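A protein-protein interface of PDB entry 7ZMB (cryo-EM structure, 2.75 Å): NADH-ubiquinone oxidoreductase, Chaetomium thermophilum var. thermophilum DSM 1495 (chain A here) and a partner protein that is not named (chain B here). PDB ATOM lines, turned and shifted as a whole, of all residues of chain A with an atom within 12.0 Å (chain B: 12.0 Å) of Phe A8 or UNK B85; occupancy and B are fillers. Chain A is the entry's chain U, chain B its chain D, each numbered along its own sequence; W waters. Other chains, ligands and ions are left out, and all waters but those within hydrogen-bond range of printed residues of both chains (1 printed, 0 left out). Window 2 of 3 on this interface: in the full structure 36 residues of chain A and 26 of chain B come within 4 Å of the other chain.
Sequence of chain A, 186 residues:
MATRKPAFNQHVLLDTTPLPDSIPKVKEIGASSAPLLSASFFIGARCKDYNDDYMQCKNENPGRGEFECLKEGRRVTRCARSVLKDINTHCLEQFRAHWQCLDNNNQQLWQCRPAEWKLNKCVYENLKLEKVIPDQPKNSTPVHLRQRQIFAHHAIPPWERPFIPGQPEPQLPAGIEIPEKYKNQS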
ATOM      1  N   MET A   1      -6.827 -26.928  18.301  1.00  0.00           N
ATOM      2  CA  MET A   1      -5.683 -26.039  18.608  1.00  0.00           C
ATOM      3  C   MET A   1      -5.812 -25.510  20.033  1.00  0.00           C
ATOM      4  O   MET A   1      -6.912 -25.613  20.583  1.00  0.00           O
ATOM      5  CB  MET A   1      -5.583 -24.908  17.590  1.00  0.00           C
ATOM      6  N   ALA A   2      -4.770 -24.878  20.570  1.00  0.00           N
ATOM      7  CA  ALA A   2      -4.738 -24.482  21.996  1.00  0.00           C
ATOM      8  C   ALA A   2      -5.801 -23.450  22.378  1.00  0.00           C
ATOM      9  O   ALA A   2      -6.262 -22.701  21.503  1.00  0.00           O
ATOM     10  CB  ALA A   2      -3.363 -23.987  22.324  1.00  0.00           C
ATOM     11  N   THR A   3      -6.179 -23.435  23.659  1.00  0.00           N
ATOM     12  CA  THR A   3      -7.232 -22.506  24.150  1.00  0.00           C
ATOM     13  C   THR A   3      -6.581 -21.213  24.641  1.00  0.00           C
ATOM     14  O   THR A   3      -7.312 -20.323  25.102  1.00  0.00           O
ATOM     15  CB  THR A   3      -8.122 -23.205  25.179  1.00  0.00           C
ATOM     16  OG1 THR A   3      -7.473 -23.139  26.450  1.00  0.00           O
ATOM     17  CG2 THR A   3      -8.410 -24.646  24.827  1.00  0.00           C
ATOM     18  N   ARG A   4      -5.263 -21.107  24.510  1.00  0.00           N
ATOM     19  CA  ARG A   4      -4.561 -19.870  24.905  1.00  0.00           C
ATOM     20  C   ARG A   4      -5.011 -18.765  23.962  1.00  0.00           C
ATOM     21  O   ARG A   4      -5.230 -19.045  22.779  1.00  0.00           O
ATOM     22  CB  ARG A   4      -3.039 -20.029  24.892  1.00  0.00           C
ATOM     23  CG  ARG A   4      -2.438 -20.337  23.534  1.00  0.00           C
ATOM     24  CD  ARG A   4      -1.005 -19.867  23.507  1.00  0.00           C
ATOM     25  NE  ARG A   4      -0.430 -19.907  22.173  1.00  0.00           N
ATOM     26  CZ  ARG A   4      -0.337 -18.859  21.364  1.00  0.00           C
ATOM     27  NH1 ARG A   4       0.214 -18.988  20.171  1.00  0.00           N
ATOM     28  NH2 ARG A   4      -0.796 -17.684  21.752  1.00  0.00           N
ATOM     29  N   LYS A   5      -5.199 -17.561  24.504  1.00  0.00           N
ATOM     30  CA  LYS A   5      -5.582 -16.412  23.655  1.00  0.00           C
ATOM     31  C   LYS A   5      -4.312 -15.857  23.001  1.00  0.00           C
ATOM     32  O   LYS A   5      -3.390 -15.472  23.736  1.00  0.00           O
ATOM     33  CB  LYS A   5      -6.287 -15.381  24.530  1.00  0.00           C
ATOM     34  CG  LYS A   5      -7.340 -15.949  25.471  1.00  0.00           C
ATOM     35  CD  LYS A   5      -7.822 -14.945  26.495  1.00  0.00           C
ATOM     36  CE  LYS A   5      -6.694 -14.364  27.322  1.00  0.00           C
ATOM     37  NZ  LYS A   5      -7.181 -13.313  28.247  1.00  0.00           N
ATOM     38  N   PRO A   6      -4.237 -15.788  21.654  1.00  0.00           N
ATOM     39  CA  PRO A   6      -3.027 -15.336  20.948  1.00  0.00           C
ATOM     40  C   PRO A   6      -2.631 -13.861  21.109  1.00  0.00           C
ATOM     41  O   PRO A   6      -3.508 -13.026  21.211  1.00  0.00           O
ATOM     42  CB  PRO A   6      -3.380 -15.589  19.476  1.00  0.00           C
ATOM     43  CG  PRO A   6      -4.886 -15.539  19.429  1.00  0.00           C
ATOM     44  CD  PRO A   6      -5.317 -16.159  20.737  1.00  0.00           C
ATOM     45  N   ALA A   7      -1.327 -13.579  21.127  1.00  0.00           N
ATOM     46  CA  ALA A   7      -0.842 -12.184  21.234  1.00  0.00           C
ATOM     47  C   ALA A   7      -0.070 -11.774  19.976  1.00  0.00           C
ATOM     48  O   ALA A   7       0.054 -10.558  19.744  1.00  0.00           O
ATOM     49  CB  ALA A   7       0.020 -12.043  22.456  1.00  0.00           C
ATOM     50  N   PHE A   8       0.425 -12.738  19.200  1.00  0.00           N
ATOM     51  CA  PHE A   8       1.256 -12.410  18.012  1.00  0.00           C
ATOM     52  C   PHE A   8       0.750 -13.171  16.779  1.00  0.00           C
ATOM     53  O   PHE A   8       1.570 -13.672  16.001  1.00  0.00           O
ATOM     54  CB  PHE A   8       2.743 -12.646  18.308  1.00  0.00           C
ATOM     55  CG  PHE A   8       3.306 -11.766  19.396  1.00  0.00           C
ATOM     56  CD1 PHE A   8       3.676 -10.459  19.138  1.00  0.00           C
ATOM     57  CD2 PHE A   8       3.451 -12.237  20.686  1.00  0.00           C
ATOM     58  CE1 PHE A   8       4.189  -9.654  20.142  1.00  0.00           C
ATOM     59  CE2 PHE A   8       3.960 -11.433  21.692  1.00  0.00           C
ATOM     60  CZ  PHE A   8       4.330 -10.140  21.418  1.00  0.00           C
ATOM     61  N   ASN A   9      -0.568 -13.237  16.606  1.00  0.00           N
ATOM     62  CA  ASN A   9      -1.179 -13.990  15.476  1.00  0.00           C
ATOM     63  C   ASN A   9      -1.298 -13.112  14.226  1.00  0.00           C
ATOM     64  O   ASN A   9      -2.132 -12.219  14.217  1.00  0.00           O
ATOM     65  CB  ASN A   9      -2.561 -14.531  15.852  1.00  0.00           C
ATOM     66  CG  ASN A   9      -3.476 -13.511  16.500  1.00  0.00           C
ATOM     67  OD1 ASN A   9      -3.087 -12.823  17.437  1.00  0.00           O
ATOM     68  ND2 ASN A   9      -4.703 -13.421  16.020  1.00  0.00           N
ATOM     69  N   GLN A  10      -0.466 -13.348  13.221  1.00  0.00           N
ATOM     70  CA  GLN A  10      -0.541 -12.561  11.964  1.00  0.00           C
ATOM     71  C   GLN A  10      -1.094 -13.438  10.840  1.00  0.00           C
ATOM     72  O   GLN A  10      -1.238 -12.931   9.721  1.00  0.00           O
ATOM     73  CB  GLN A  10       0.840 -11.996  11.624  1.00  0.00           C
ATOM     74  CG  GLN A  10       1.566 -11.351  12.798  1.00  0.00           C
ATOM     75  CD  GLN A  10       1.022  -9.995  13.184  1.00  0.00           C
ATOM     76  OE1 GLN A  10      -0.180  -9.806  13.361  1.00  0.00           O
ATOM     77  NE2 GLN A  10       1.916  -9.037  13.343  1.00  0.00           N
ATOM     78  N   HIS A  11      -1.435 -14.694  11.141  1.00  0.00           N
ATOM     79  CA  HIS A  11      -1.865 -15.643  10.081  1.00  0.00           C
ATOM     80  C   HIS A  11      -3.008 -16.529  10.553  1.00  0.00           C
ATOM     81  O   HIS A  11      -3.183 -16.658  11.773  1.00  0.00           O
ATOM     82  CB  HIS A  11      -0.681 -16.509   9.622  1.00  0.00           C
ATOM     83  CG  HIS A  11       0.418 -15.725   8.994  1.00  0.00           C
ATOM     84  ND1 HIS A  11       0.287 -15.150   7.749  1.00  0.00           N
ATOM     85  CD2 HIS A  11       1.652 -15.403   9.437  1.00  0.00           C
ATOM     86  CE1 HIS A  11       1.399 -14.515   7.441  1.00  0.00           C
ATOM     87  NE2 HIS A  11       2.253 -14.657   8.462  1.00  0.00           N
ATOM     88  N   VAL A  12      -3.745 -17.113   9.611  1.00  0.00           N
ATOM     89  CA  VAL A  12      -4.867 -18.040   9.938  1.00  0.00           C
ATOM     90  C   VAL A  12      -4.658 -19.320   9.119  1.00  0.00           C
ATOM     91  O   VAL A  12      -4.192 -19.213   7.974  1.00  0.00           O
ATOM     92  CB  VAL A  12      -6.223 -17.369   9.642  1.00  0.00           C
ATOM     93  CG1 VAL A  12      -7.348 -18.373   9.456  1.00  0.00           C
ATOM     94  CG2 VAL A  12      -6.597 -16.349  10.705  1.00  0.00           C
ATOM     95  N   LEU A  13      -4.960 -20.486   9.696  1.00  0.00           N
ATOM     96  CA  LEU A  13      -4.802 -21.776   8.980  1.00  0.00           C
ATOM     97  C   LEU A  13      -6.147 -22.486   8.832  1.00  0.00           C
ATOM     98  O   LEU A  13      -6.840 -22.629   9.846  1.00  0.00           O
ATOM     99  CB  LEU A  13      -3.798 -22.649   9.734  1.00  0.00           C
ATOM    100  CG  LEU A  13      -3.406 -23.961   9.058  1.00  0.00           C
ATOM    101  CD1 LEU A  13      -2.745 -23.708   7.714  1.00  0.00           C
ATOM    102  CD2 LEU A  13      -2.480 -24.757   9.957  1.00  0.00           C
ATOM    103  N   GLN B  44     -13.366 -12.667  25.971  1.00  0.00           N
ATOM    104  CA  GLN B  44     -13.025 -13.735  25.005  1.00  0.00           C
ATOM    105  C   GLN B  44     -14.289 -14.240  24.310  1.00  0.00           C
ATOM    106  O   GLN B  44     -14.191 -14.591  23.133  1.00  0.00           O
ATOM    107  CB  GLN B  44     -12.251 -14.843  25.719  1.00  0.00           C
ATOM    108  CG  GLN B  44     -11.627 -15.869  24.785  1.00  0.00           C
ATOM    109  CD  GLN B  44     -10.830 -15.259  23.654  1.00  0.00           C
ATOM    110  OE1 GLN B  44     -10.877 -15.726  22.520  1.00  0.00           O
ATOM    111  NE2 GLN B  44     -10.086 -14.205  23.951  1.00  0.00           N
ATOM    112  N   GLU B  51     -15.898 -13.014  15.601  1.00  0.00           N
ATOM    113  CA  GLU B  51     -15.149 -13.718  14.541  1.00  0.00           C
ATOM    114  C   GLU B  51     -16.116 -14.712  13.911  1.00  0.00           C
ATOM    115  O   GLU B  51     -15.975 -14.979  12.712  1.00  0.00           O
ATOM    116  CB  GLU B  51     -13.961 -14.452  15.147  1.00  0.00           C
ATOM    117  CG  GLU B  51     -12.815 -13.546  15.541  1.00  0.00           C
ATOM    118  CD  GLU B  51     -11.820 -14.233  16.460  1.00  0.00           C
ATOM    119  OE1 GLU B  51     -12.239 -15.148  17.192  1.00  0.00           O
ATOM    120  OE2 GLU B  51     -10.632 -13.861  16.427  1.00  0.00           O
ATOM    121  N   TRP B  79      -8.081 -20.886  12.378  1.00  0.00           N
ATOM    122  CA  TRP B  79      -7.137 -21.375  13.416  1.00  0.00           C
ATOM    123  C   TRP B  79      -5.984 -20.377  13.403  1.00  0.00           C
ATOM    124  O   TRP B  79      -5.413 -20.175  12.332  1.00  0.00           O
ATOM    125  CB  TRP B  79      -6.717 -22.826  13.188  1.00  0.00           C
ATOM    126  CG  TRP B  79      -7.614 -23.829  13.845  1.00  0.00           C
ATOM    127  CD1 TRP B  79      -8.894 -23.637  14.273  1.00  0.00           C
ATOM    128  CD2 TRP B  79      -7.295 -25.200  14.143  1.00  0.00           C
ATOM    129  NE1 TRP B  79      -9.391 -24.787  14.822  1.00  0.00           N
ATOM    130  CE2 TRP B  79      -8.434 -25.763  14.755  1.00  0.00           C
ATOM    131  CE3 TRP B  79      -6.165 -26.002  13.955  1.00  0.00           C
ATOM    132  CZ2 TRP B  79      -8.472 -27.091  15.177  1.00  0.00           C
ATOM    133  CZ3 TRP B  79      -6.201 -27.313  14.376  1.00  0.00           C
ATOM    134  CH2 TRP B  79      -7.341 -27.847  14.976  1.00  0.00           C
ATOM    135  N   LYS B  80      -5.644 -19.786  14.540  1.00  0.00           N
ATOM    136  CA  LYS B  80      -4.692 -18.687  14.549  1.00  0.00           C
ATOM    137  C   LYS B  80      -3.262 -19.218  14.560  1.00  0.00           C
ATOM    138  O   LYS B  80      -2.944 -20.170  15.272  1.00  0.00           O
ATOM    139  CB  LYS B  80      -4.940 -17.809  15.771  1.00  0.00           C
ATOM    140  CG  LYS B  80      -6.329 -17.232  15.800  1.00  0.00           C
ATOM    141  CD  LYS B  80      -6.579 -16.282  14.693  1.00  0.00           C
ATOM    142  CE  LYS B  80      -7.927 -15.624  14.867  1.00  0.00           C
ATOM    143  NZ  LYS B  80      -9.022 -16.599  14.655  1.00  0.00           N
ATOM    144  N   VAL B  81      -2.376 -18.609  13.770  1.00  0.00           N
ATOM    145  CA  VAL B  81      -0.954 -19.066  13.671  1.00  0.00           C
ATOM    146  C   VAL B  81      -0.015 -17.977  14.199  1.00  0.00           C
ATOM    147  O   VAL B  81      -0.148 -16.826  13.759  1.00  0.00           O
ATOM    148  CB  VAL B  81      -0.596 -19.473  12.228  1.00  0.00           C
ATOM    149  CG1 VAL B  81       0.901 -19.546  11.992  1.00  0.00           C
ATOM    150  CG2 VAL B  81      -1.275 -20.762  11.802  1.00  0.00           C
ATOM    151  N   UNK B  82       0.886 -18.328  15.122  1.00  0.00           N
ATOM    152  CA  UNK B  82       1.860 -17.365  15.688  1.00  0.00           C
ATOM    153  C   UNK B  82       3.269 -17.959  15.641  1.00  0.00           C
ATOM    154  O   UNK B  82       3.396 -19.178  15.791  1.00  0.00           O
ATOM    155  CB  UNK B  82       1.477 -17.000  17.103  1.00  0.00           C
ATOM    156  N   UNK B  83       4.279 -17.140  15.355  1.00  0.00           N
ATOM    157  CA  UNK B  83       5.675 -17.629  15.434  1.00  0.00           C
ATOM    158  C   UNK B  83       6.176 -17.836  16.871  1.00  0.00           C
ATOM    159  O   UNK B  83       6.870 -18.843  17.080  1.00  0.00           O
ATOM    160  CB  UNK B  83       6.601 -16.766  14.615  1.00  0.00           C
ATOM    161  N   UNK B  84       5.837 -16.951  17.825  1.00  0.00           N
ATOM    162  CA  UNK B  84       6.494 -17.050  19.155  1.00  0.00           C
ATOM    163  C   UNK B  84       5.665 -17.148  20.440  1.00  0.00           C
ATOM    164  O   UNK B  84       5.980 -18.052  21.241  1.00  0.00           O
ATOM    165  CB  UNK B  84       7.516 -15.946  19.306  1.00  0.00           C
ATOM    166  N   UNK B  85       4.682 -16.279  20.682  1.00  0.00           N
ATOM    167  CA  UNK B  85       4.083 -16.247  22.048  1.00  0.00           C
ATOM    168  C   UNK B  85       3.003 -17.269  22.363  1.00  0.00           C
ATOM    169  O   UNK B  85       1.827 -16.899  22.376  1.00  0.00           O
ATOM    170  CB  UNK B  85       3.697 -14.871  22.489  1.00  0.00           C
ATOM    171  N   UNK B  86       3.422 -18.490  22.669  1.00  0.00           N
ATOM    172  CA  UNK B  86       2.474 -19.504  23.153  1.00  0.00           C
ATOM    173  C   UNK B  86       2.198 -19.198  24.630  1.00  0.00           C
ATOM    174  O   UNK B  86       3.023 -18.478  25.227  1.00  0.00           O
ATOM    175  CB  UNK B  86       3.067 -20.872  22.974  1.00  0.00           C
HETATM  176  O   HOH W   1      -0.417 -16.497  24.688  1.00  0.00           O
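Water W1 lies within hydrogen-bond range of NH2 of Arg A4, O of UNK B85 and O of Lys A5.
Among the printed residues, merely in contact across the chains: Arg A4 with UNK B86 (3.1 Å), Phe A8 with UNK B85 (3.2 Å), Val A12 with Trp B79 (3.3 Å), Asn A9 with Val B81 (3.5 Å), Lys A5 with Gln B44 (3.5 Å), Met A1 with Trp B79 (3.5 Å), Phe A8 with UNK B82 (3.5 Å), Gln A10 with Val B81 (3.5 Å), Asn A9 with Lys B80 (3.7 Å), His A11 with Lys B80 (3.8 Å), Leu A13 with Val B81 (3.8 Å), Arg A4 with UNK B82 (3.9 Å) and Val A12 with Lys B80 (3.99 Å).
Of the printed residues of chain B, Phe A8 touches UNK B82 and UNK B85.
No residue of chain B comes within 4 Å of Pro A6.
Asn A9 touches two residues of chain B.
No residue of chain A comes within 4 Å of UNK B83.
Of the printed residues of chain B, His A11 touches Lys B80 (3.8 Å) and Val B81 (2.9 Å).
Of the printed residues of chain B, Lys A5 touches Gln B44.
Printed residues of chain B within 4 Å of Arg A4: UNK B82 (3.9 Å), UNK B85 (2.8 Å) and UNK B86 (3.1 Å).
Printed residues of chain A within 4 Å of Val B81: Asn A9, Gln A10, His A11 and Leu A13.
Of the printed residues of chain B, Met A1 touches Trp B79.
Thr A3 touches none of the printed residues of chain B.
The nearest printed residue of chain A that does not touch Val B81 is Phe A8 (4.2 Å).
Printed residues of chain B that touch a printed residue of chain A: Gln B44, Trp B79, Lys B80, Val B81, UNK B82, UNK B85 and UNK B86.
Among the printed residues, 16 pairs touch across the chains.
Among the printed residues, no Asp or Glu carboxylate lies within 4 Å of a Lys or Arg side-chain nitrogen of the other chain.
The backbone carbonyl oxygen (O) of Trp B79 sits at hydrogen-bond distance from the backbone NH (N) of Leu A13.
O of His A11 sits at hydrogen-bond distance from N of Val B81 (2.9 Å).
O of UNK B85 sits at hydrogen-bond distance from NH2 of Arg A4, at 2.8 Å.
The side-chain carboxylate (OE2) of Glu B51 is in salt-bridge range of the side-chain amino group (NZ) of Lys B80.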
